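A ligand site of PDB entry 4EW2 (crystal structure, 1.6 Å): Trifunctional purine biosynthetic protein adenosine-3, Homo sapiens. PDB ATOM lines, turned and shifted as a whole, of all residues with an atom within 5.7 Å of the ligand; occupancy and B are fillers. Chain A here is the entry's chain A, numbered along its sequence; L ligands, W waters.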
ATOM      1  N   ASN A  36      35.895  15.568  -4.832  1.00  0.00           N
ATOM      2  CA  ASN A  36      35.759  14.276  -4.186  1.00  0.00           C
ATOM      3  C   ASN A  36      35.827  13.138  -5.200  1.00  0.00           C
ATOM      4  O   ASN A  36      35.795  11.962  -4.820  1.00  0.00           O
ATOM      5  CB  ASN A  36      34.485  14.137  -3.359  1.00  0.00           C
ATOM      6  CG  ASN A  36      33.260  14.222  -4.199  1.00  0.00           C
ATOM      7  OD1 ASN A  36      33.086  15.190  -4.917  1.00  0.00           O
ATOM      8  ND2 ASN A  36      32.417  13.176  -4.153  1.00  0.00           N
ATOM      9  N   LYS A  37      36.008  13.507  -6.456  1.00  0.00           N
ATOM     10  CA  LYS A  37      36.080  12.521  -7.549  1.00  0.00           C
ATOM     11  C   LYS A  37      37.264  12.783  -8.461  1.00  0.00           C
ATOM     12  O   LYS A  37      37.475  13.884  -8.924  1.00  0.00           O
ATOM     13  CB  LYS A  37      34.771  12.522  -8.348  1.00  0.00           C
ATOM     14  CG  LYS A  37      33.598  12.018  -7.559  1.00  0.00           C
ATOM     15  CD  LYS A  37      32.382  11.843  -8.399  1.00  0.00           C
ATOM     16  CE  LYS A  37      31.625  10.626  -7.953  1.00  0.00           C
ATOM     17  NZ  LYS A  37      32.424   9.379  -8.205  1.00  0.00           N
ATOM     18  N   ARG A  64      30.782  10.837   7.281  1.00  0.00           N
ATOM     19  CA  ARG A  64      30.733  12.164   6.672  1.00  0.00           C
ATOM     20  C   ARG A  64      31.607  13.167   7.424  1.00  0.00           C
ATOM     21  O   ARG A  64      32.298  14.008   6.841  1.00  0.00           O
ATOM     22  CB  ARG A  64      29.270  12.615   6.596  1.00  0.00           C
ATOM     23  CG  ARG A  64      28.971  13.959   5.990  1.00  0.00           C
ATOM     24  CD  ARG A  64      27.421  14.151   5.729  1.00  0.00           C
ATOM     25  NE  ARG A  64      26.794  12.942   5.162  1.00  0.00           N
ATOM     26  CZ  ARG A  64      26.688  12.625   3.863  1.00  0.00           C
ATOM     27  NH1 ARG A  64      27.146  13.423   2.888  1.00  0.00           N
ATOM     28  NH2 ARG A  64      26.078  11.460   3.522  1.00  0.00           N
ATOM     29  N   LEU A  85      31.241  26.553  -3.625  1.00  0.00           N
ATOM     30  CA  LEU A  85      30.825  25.223  -4.126  1.00  0.00           C
ATOM     31  C   LEU A  85      30.464  25.388  -5.575  1.00  0.00           C
ATOM     32  O   LEU A  85      29.698  26.297  -5.965  1.00  0.00           O
ATOM     33  CB  LEU A  85      29.661  24.646  -3.328  1.00  0.00           C
ATOM     34  CG  LEU A  85      29.764  24.522  -1.805  1.00  0.00           C
ATOM     35  CD1 LEU A  85      28.541  23.822  -1.229  1.00  0.00           C
ATOM     36  CD2 LEU A  85      31.062  23.778  -1.354  1.00  0.00           C
ATOM     37  N   PHE A  88      29.323  20.587  -6.093  1.00  0.00           N
ATOM     38  CA  PHE A  88      29.796  19.661  -5.086  1.00  0.00           C
ATOM     39  C   PHE A  88      28.657  18.805  -4.586  1.00  0.00           C
ATOM     40  O   PHE A  88      27.688  19.320  -4.019  1.00  0.00           O
ATOM     41  CB  PHE A  88      30.492  20.409  -3.943  1.00  0.00           C
ATOM     42  CG  PHE A  88      31.146  19.496  -2.955  1.00  0.00           C
ATOM     43  CD1 PHE A  88      32.284  18.796  -3.293  1.00  0.00           C
ATOM     44  CD2 PHE A  88      30.634  19.337  -1.705  1.00  0.00           C
ATOM     45  CE1 PHE A  88      32.877  17.972  -2.397  1.00  0.00           C
ATOM     46  CE2 PHE A  88      31.231  18.511  -0.785  1.00  0.00           C
ATOM     47  CZ  PHE A  88      32.365  17.812  -1.148  1.00  0.00           C
ATOM     48  N   MET A  89      28.742  17.497  -4.775  1.00  0.00           N
ATOM     49  CA  MET A  89      27.576  16.611  -4.607  1.00  0.00           C
ATOM     50  C   MET A  89      27.521  15.789  -3.350  1.00  0.00           C
ATOM     51  O   MET A  89      26.798  14.779  -3.273  1.00  0.00           O
ATOM     52  CB  MET A  89      27.444  15.728  -5.852  1.00  0.00           C
ATOM     53  CG  MET A  89      27.340  16.527  -7.127  1.00  0.00           C
ATOM     54  SD  MET A  89      25.969  17.742  -7.199  1.00  0.00           S
ATOM     55  CE  MET A  89      24.648  16.573  -7.034  1.00  0.00           C
ATOM     56  N   ARG A  90      28.276  16.209  -2.335  1.00  0.00           N
ATOM     57  CA  ARG A  90      28.176  15.578  -1.034  1.00  0.00           C
ATOM     58  C   ARG A  90      27.655  16.607  -0.052  1.00  0.00           C
ATOM     59  O   ARG A  90      28.153  17.724  -0.007  1.00  0.00           O
ATOM     60  CB  ARG A  90      29.531  15.041  -0.551  1.00  0.00           C
ATOM     61  CG  ARG A  90      30.208  14.112  -1.529  1.00  0.00           C
ATOM     62  CD  ARG A  90      29.470  12.805  -1.644  1.00  0.00           C
ATOM     63  NE  ARG A  90      29.372  12.068  -0.396  1.00  0.00           N
ATOM     64  CZ  ARG A  90      28.829  10.872  -0.277  1.00  0.00           C
ATOM     65  NH1 ARG A  90      28.320  10.294  -1.347  1.00  0.00           N
ATOM     66  NH2 ARG A  90      28.785  10.278   0.899  1.00  0.00           N
ATOM     67  N   ILE A  91      26.666  16.197   0.736  1.00  0.00           N
ATOM     68  CA  ILE A  91      26.136  17.034   1.813  1.00  0.00           C
ATOM     69  C   ILE A  91      27.219  17.198   2.866  1.00  0.00           C
ATOM     70  O   ILE A  91      27.782  16.216   3.371  1.00  0.00           O
ATOM     71  CB  ILE A  91      24.867  16.424   2.463  1.00  0.00           C
ATOM     72  CG1 ILE A  91      23.739  16.304   1.441  1.00  0.00           C
ATOM     73  CG2 ILE A  91      24.394  17.285   3.607  1.00  0.00           C
ATOM     74  CD1 ILE A  91      23.259  17.617   0.939  1.00  0.00           C
ATOM     75  N   LEU A  92      27.546  18.446   3.138  1.00  0.00           N
ATOM     76  CA  LEU A  92      28.535  18.804   4.147  1.00  0.00           C
ATOM     77  C   LEU A  92      27.920  18.769   5.536  1.00  0.00           C
ATOM     78  O   LEU A  92      26.783  19.222   5.732  1.00  0.00           O
ATOM     79  CB  LEU A  92      29.131  20.173   3.861  1.00  0.00           C
ATOM     80  CG  LEU A  92      30.020  20.215   2.606  1.00  0.00           C
ATOM     81  CD1 LEU A  92      30.136  21.646   2.057  1.00  0.00           C
ATOM     82  CD2 LEU A  92      31.403  19.568   2.847  1.00  0.00           C
ATOM     83  N   SER A  93      28.679  18.213   6.480  1.00  0.00           N
ATOM     84  CA  SER A  93      28.258  18.023   7.861  1.00  0.00           C
ATOM     85  C   SER A  93      27.942  19.344   8.545  1.00  0.00           C
ATOM     86  O   SER A  93      28.412  20.408   8.176  1.00  0.00           O
ATOM     87  CB  SER A  93      29.356  17.316   8.672  1.00  0.00           C
ATOM     88  OG  SER A  93      30.464  18.188   8.910  1.00  0.00           O
ATOM     89  N   VAL A  97      29.806  23.043   8.079  1.00  0.00           N
ATOM     90  CA  VAL A  97      29.041  24.215   7.646  1.00  0.00           C
ATOM     91  C   VAL A  97      29.119  25.349   8.674  1.00  0.00           C
ATOM     92  O   VAL A  97      29.292  26.510   8.329  1.00  0.00           O
ATOM     93  CB  VAL A  97      27.562  23.847   7.349  1.00  0.00           C
ATOM     94  CG1 VAL A  97      26.759  25.115   7.047  1.00  0.00           C
ATOM     95  CG2 VAL A  97      27.480  22.879   6.161  1.00  0.00           C
ATOM     96  N   ASN A 106      27.408  29.307  -2.548  1.00  0.00           N
ATOM     97  CA  ASN A 106      27.042  28.475  -3.656  1.00  0.00           C
ATOM     98  C   ASN A 106      25.991  29.126  -4.527  1.00  0.00           C
ATOM     99  O   ASN A 106      25.529  30.228  -4.201  1.00  0.00           O
ATOM    100  CB  ASN A 106      26.682  27.084  -3.194  1.00  0.00           C
ATOM    101  CG  ASN A 106      25.357  26.961  -2.611  1.00  0.00           C
ATOM    102  OD1 ASN A 106      24.718  25.871  -2.724  1.00  0.00           O
ATOM    103  ND2 ASN A 106      24.912  27.988  -1.944  1.00  0.00           N
ATOM    104  N   GLY A 117      15.865  22.228  -4.975  1.00  0.00           N
ATOM    105  CA  GLY A 117      16.256  20.910  -5.421  1.00  0.00           C
ATOM    106  C   GLY A 117      16.814  20.833  -6.818  1.00  0.00           C
ATOM    107  O   GLY A 117      17.221  21.815  -7.437  1.00  0.00           O
ATOM    108  N   SER A 118      16.829  19.621  -7.350  1.00  0.00           N
ATOM    109  CA  SER A 118      17.427  19.424  -8.653  1.00  0.00           C
ATOM    110  C   SER A 118      16.446  19.764  -9.764  1.00  0.00           C
ATOM    111  O   SER A 118      15.240  19.943  -9.538  1.00  0.00           O
ATOM    112  CB  SER A 118      17.914  17.976  -8.789  1.00  0.00           C
ATOM    113  OG  SER A 118      16.910  17.136  -8.335  1.00  0.00           O
ATOM    114  N   HIS A 137      24.041  32.295  -2.622  1.00  0.00           N
ATOM    115  CA  HIS A 137      23.790  32.362  -1.198  1.00  0.00           C
ATOM    116  C   HIS A 137      24.894  31.753  -0.369  1.00  0.00           C
ATOM    117  O   HIS A 137      25.642  30.927  -0.843  1.00  0.00           O
ATOM    118  CB  HIS A 137      22.439  31.727  -0.855  1.00  0.00           C
ATOM    119  CG  HIS A 137      22.343  30.271  -1.170  1.00  0.00           C
ATOM    120  ND1 HIS A 137      22.564  29.288  -0.231  1.00  0.00           N
ATOM    121  CD2 HIS A 137      21.973  29.633  -2.309  1.00  0.00           C
ATOM    122  CE1 HIS A 137      22.352  28.107  -0.775  1.00  0.00           C
ATOM    123  NE2 HIS A 137      21.975  28.287  -2.032  1.00  0.00           N
ATOM    124  N   VAL A 139      26.102  29.134   2.193  1.00  0.00           N
ATOM    125  CA  VAL A 139      25.706  27.775   2.446  1.00  0.00           C
ATOM    126  C   VAL A 139      25.305  27.523   3.901  1.00  0.00           C
ATOM    127  O   VAL A 139      25.984  27.963   4.860  1.00  0.00           O
ATOM    128  CB  VAL A 139      26.861  26.813   2.057  1.00  0.00           C
ATOM    129  CG1 VAL A 139      26.507  25.392   2.439  1.00  0.00           C
ATOM    130  CG2 VAL A 139      27.159  26.937   0.553  1.00  0.00           C
ATOM    131  N   ALA A 140      24.162  26.867   4.032  1.00  0.00           N
ATOM    132  CA  ALA A 140      23.617  26.426   5.319  1.00  0.00           C
ATOM    133  C   ALA A 140      23.544  24.930   5.409  1.00  0.00           C
ATOM    134  O   ALA A 140      23.790  24.228   4.412  1.00  0.00           O
ATOM    135  CB  ALA A 140      22.171  27.020   5.500  1.00  0.00           C
ATOM    136  N   GLU A 141      23.223  24.411   6.580  1.00  0.00           N
ATOM    137  CA  GLU A 141      23.185  22.949   6.772  1.00  0.00           C
ATOM    138  C   GLU A 141      22.134  22.320   5.851  1.00  0.00           C
ATOM    139  O   GLU A 141      22.360  21.263   5.210  1.00  0.00           O
ATOM    140  CB  GLU A 141      22.962  22.552   8.243  1.00  0.00           C
ATOM    141  CG  GLU A 141      24.122  22.949   9.120  1.00  0.00           C
ATOM    142  CD  GLU A 141      24.037  22.532  10.618  1.00  0.00           C
ATOM    143  OE1 GLU A 141      23.318  21.556  10.954  1.00  0.00           O
ATOM    144  OE2 GLU A 141      24.731  23.181  11.445  1.00  0.00           O
ATOM    145  N   ASP A 142      20.980  22.972   5.795  1.00  0.00           N
ATOM    146  CA  ASP A 142      19.906  22.565   4.878  1.00  0.00           C
ATOM    147  C   ASP A 142      20.167  23.048   3.462  1.00  0.00           C
ATOM    148  O   ASP A 142      20.420  24.217   3.227  1.00  0.00           O
ATOM    149  CB  ASP A 142      18.571  23.214   5.277  1.00  0.00           C
ATOM    150  CG  ASP A 142      17.925  22.533   6.418  1.00  0.00           C
ATOM    151  OD1 ASP A 142      18.433  21.502   6.895  1.00  0.00           O
ATOM    152  OD2 ASP A 142      16.855  23.050   6.813  1.00  0.00           O
ATOM    153  N   VAL A 143      20.031  22.136   2.509  1.00  0.00           N
ATOM    154  CA  VAL A 143      20.185  22.470   1.099  1.00  0.00           C
ATOM    155  C   VAL A 143      19.201  23.584   0.688  1.00  0.00           C
ATOM    156  O   VAL A 143      18.029  23.579   1.103  1.00  0.00           O
ATOM    157  CB  VAL A 143      19.988  21.223   0.214  1.00  0.00           C
ATOM    158  CG1 VAL A 143      19.977  21.593  -1.290  1.00  0.00           C
ATOM    159  CG2 VAL A 143      21.120  20.205   0.510  1.00  0.00           C
ATOM    160  N   ASP A 144      19.687  24.528  -0.110  1.00  0.00           N
ATOM    161  CA  ASP A 144      18.890  25.672  -0.638  1.00  0.00           C
ATOM    162  C   ASP A 144      18.533  26.770   0.390  1.00  0.00           C
ATOM    163  O   ASP A 144      18.025  27.853   0.001  1.00  0.00           O
ATOM    164  CB  ASP A 144      17.600  25.188  -1.324  1.00  0.00           C
ATOM    165  CG  ASP A 144      17.881  24.439  -2.594  1.00  0.00           C
ATOM    166  OD1 ASP A 144      18.802  24.838  -3.333  1.00  0.00           O
ATOM    167  OD2 ASP A 144      17.195  23.429  -2.847  1.00  0.00           O
ATOM    168  N   ALA A 145      18.757  26.490   1.668  1.00  0.00           N
ATOM    169  CA  ALA A 145      18.619  27.500   2.724  1.00  0.00           C
ATOM    170  C   ALA A 145      19.942  28.262   2.759  1.00  0.00           C
ATOM    171  O   ALA A 145      20.895  27.897   2.082  1.00  0.00           O
ATOM    172  CB  ALA A 145      18.388  26.864   4.087  1.00  0.00           C
HETATM  173  O1  LIG L   1      27.520  11.839  -4.412  1.00  0.00           O
HETATM  174  C1  LIG L   1      26.300  11.510  -4.568  1.00  0.00           C
HETATM  175  O2  LIG L   1      25.891  10.596  -5.327  1.00  0.00           O
HETATM  176  C2  LIG L   1      25.186  12.293  -3.774  1.00  0.00           C
HETATM  177  C3  LIG L   1      25.052  11.768  -2.326  1.00  0.00           C
HETATM  178  C4  LIG L   1      24.312  12.703  -1.336  1.00  0.00           C
HETATM  179  C5  LIG L   1      25.060  12.624   0.005  1.00  0.00           C
HETATM  180  O3  LIG L   1      25.867  13.517   0.293  1.00  0.00           O
HETATM  181  O4  LIG L   1      24.823  11.615   0.695  1.00  0.00           O
HETATM  182  N1  LIG L   1      24.159  14.096  -1.840  1.00  0.00           N
HETATM  183  C6  LIG L   1      22.975  14.711  -1.790  1.00  0.00           C
HETATM  184  O5  LIG L   1      21.959  14.161  -1.393  1.00  0.00           O
HETATM  185  C7  LIG L   1      22.976  16.093  -2.375  1.00  0.00           C
HETATM  186  C8  LIG L   1      21.885  16.962  -2.483  1.00  0.00           C
HETATM  187  C9  LIG L   1      22.017  18.225  -3.059  1.00  0.00           C
HETATM  188  C10 LIG L   1      24.182  16.526  -2.816  1.00  0.00           C
HETATM  189  C11 LIG L   1      24.317  17.765  -3.389  1.00  0.00           C
HETATM  190  C12 LIG L   1      23.253  18.646  -3.524  1.00  0.00           C
HETATM  191  C13 LIG L   1      23.632  19.993  -4.220  1.00  0.00           C
HETATM  192  S1  LIG L   1      22.769  20.189  -5.831  1.00  0.00           S
HETATM  193  C14 LIG L   1      21.330  19.125  -5.830  1.00  0.00           C
HETATM  194  C15 LIG L   1      23.618  21.286  -3.348  1.00  0.00           C
HETATM  195  C16 LIG L   1      24.236  21.107  -1.970  1.00  0.00           C
HETATM  196  C17 LIG L   1      25.142  22.246  -1.391  1.00  0.00           C
HETATM  197  C18 LIG L   1      25.203  21.966   0.088  1.00  0.00           C
HETATM  198  C19 LIG L   1      24.368  22.608   0.992  1.00  0.00           C
HETATM  199  O6  LIG L   1      23.590  23.489   0.660  1.00  0.00           O
HETATM  200  N2  LIG L   1      24.407  22.291   2.304  1.00  0.00           N
HETATM  201  C20 LIG L   1      25.250  21.315   2.769  1.00  0.00           C
HETATM  202  N3  LIG L   1      25.215  21.048   4.055  1.00  0.00           N
HETATM  203  N4  LIG L   1      26.054  20.668   1.915  1.00  0.00           N
HETATM  204  C21 LIG L   1      26.063  20.963   0.616  1.00  0.00           C
HETATM  205  N5  LIG L   1      26.866  20.286  -0.206  1.00  0.00           N
HETATM  206  O   HOH W   1      22.010  23.827  -3.808  1.00  0.00           O
HETATM  207  O   HOH W   2      22.302  24.752  -1.289  1.00  0.00           O
HETATM  208  O   HOH W   3      20.672  15.960  -6.217  1.00  0.00           O
HETATM  209  O   HOH W   4      22.744  26.018   1.665  1.00  0.00           O
HETATM  210  O   HOH W   5      29.880  12.915  -5.545  1.00  0.00           O
HETATM  211  O   HOH W   6      25.945  12.736  -7.373  1.00  0.00           O
HETATM  212  O   HOH W   7      18.436  17.738  -4.511  1.00  0.00           O
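Water W2 lies within hydrogen-bond range of O6 of the ligand (2.7 Å), N of Asp 144 (2.9 Å) and OD1 of Asn 106 (3.0 Å). Water W5 lies within hydrogen-bond range of an oxygen (O1) of the ligand (2.8 Å) and the side-chain amide nitrogen of Asn 36 (2.9 Å).
O3 of the ligand sits at hydrogen-bond distance from N of Ile 91, 2.8 Å away. The backbone carbonyl oxygen of Arg 90 is in hydrogen-bond range of a nitrogen (N5) of the ligand, at 2.9 Å. An oxygen (O1) of the ligand is in salt-bridge range of the guanidinium group (NH1) of Arg 90. The guanidinium group of Arg 64 is in salt-bridge range of an oxygen (O3) of the ligand, at 2.9 Å. A nitrogen (N2) of the ligand lies within hydrogen-bond range of the backbone carbonyl oxygen of Ala 140, 2.9 Å away. N4 of the ligand is in hydrogen-bond range of N of Leu 92. O of Leu 92 sits at hydrogen-bond distance from N3 of the ligand, at 2.9 Å. The backbone carbonyl oxygen of Met 89 sits close to a nitrogen (N1) of the ligand (3.1 Å). A nitrogen (N3) of the ligand sits at hydrogen-bond distance from the backbone carbonyl oxygen (O) of Glu 141 (3.1 Å).
Merely in contact with the ligand: Val 143 (3.6 Å), Val 97 (3.6 Å), Val 139 (3.7 Å), Leu 85 (3.8 Å), Phe 88 (3.8 Å) and Asn 106 (3.9 Å). Hydrophobic or aromatic side chains within 4 Å of the ligand: Leu 85, Met 89, Ile 91, Leu 92, Val 97 and Val 139. Within 4 Å of the ligand: Arg 64, Leu 85, Phe 88, Met 89, Arg 90, Ile 91, Leu 92, Val 97, Asn 106, Val 139, Ala 140, Glu 141 and Val 143. The nearest printed residue that does not touch the ligand is Asp 144 (4.1 Å).
The backbone carbonyl oxygen (O) of Ile 91 sits at hydrogen-bond distance from the guanidinium group (NH1) of Arg 64 (2.9 Å). O of His 137 lies within hydrogen-bond range of N of Asn 106 (2.9 Å).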
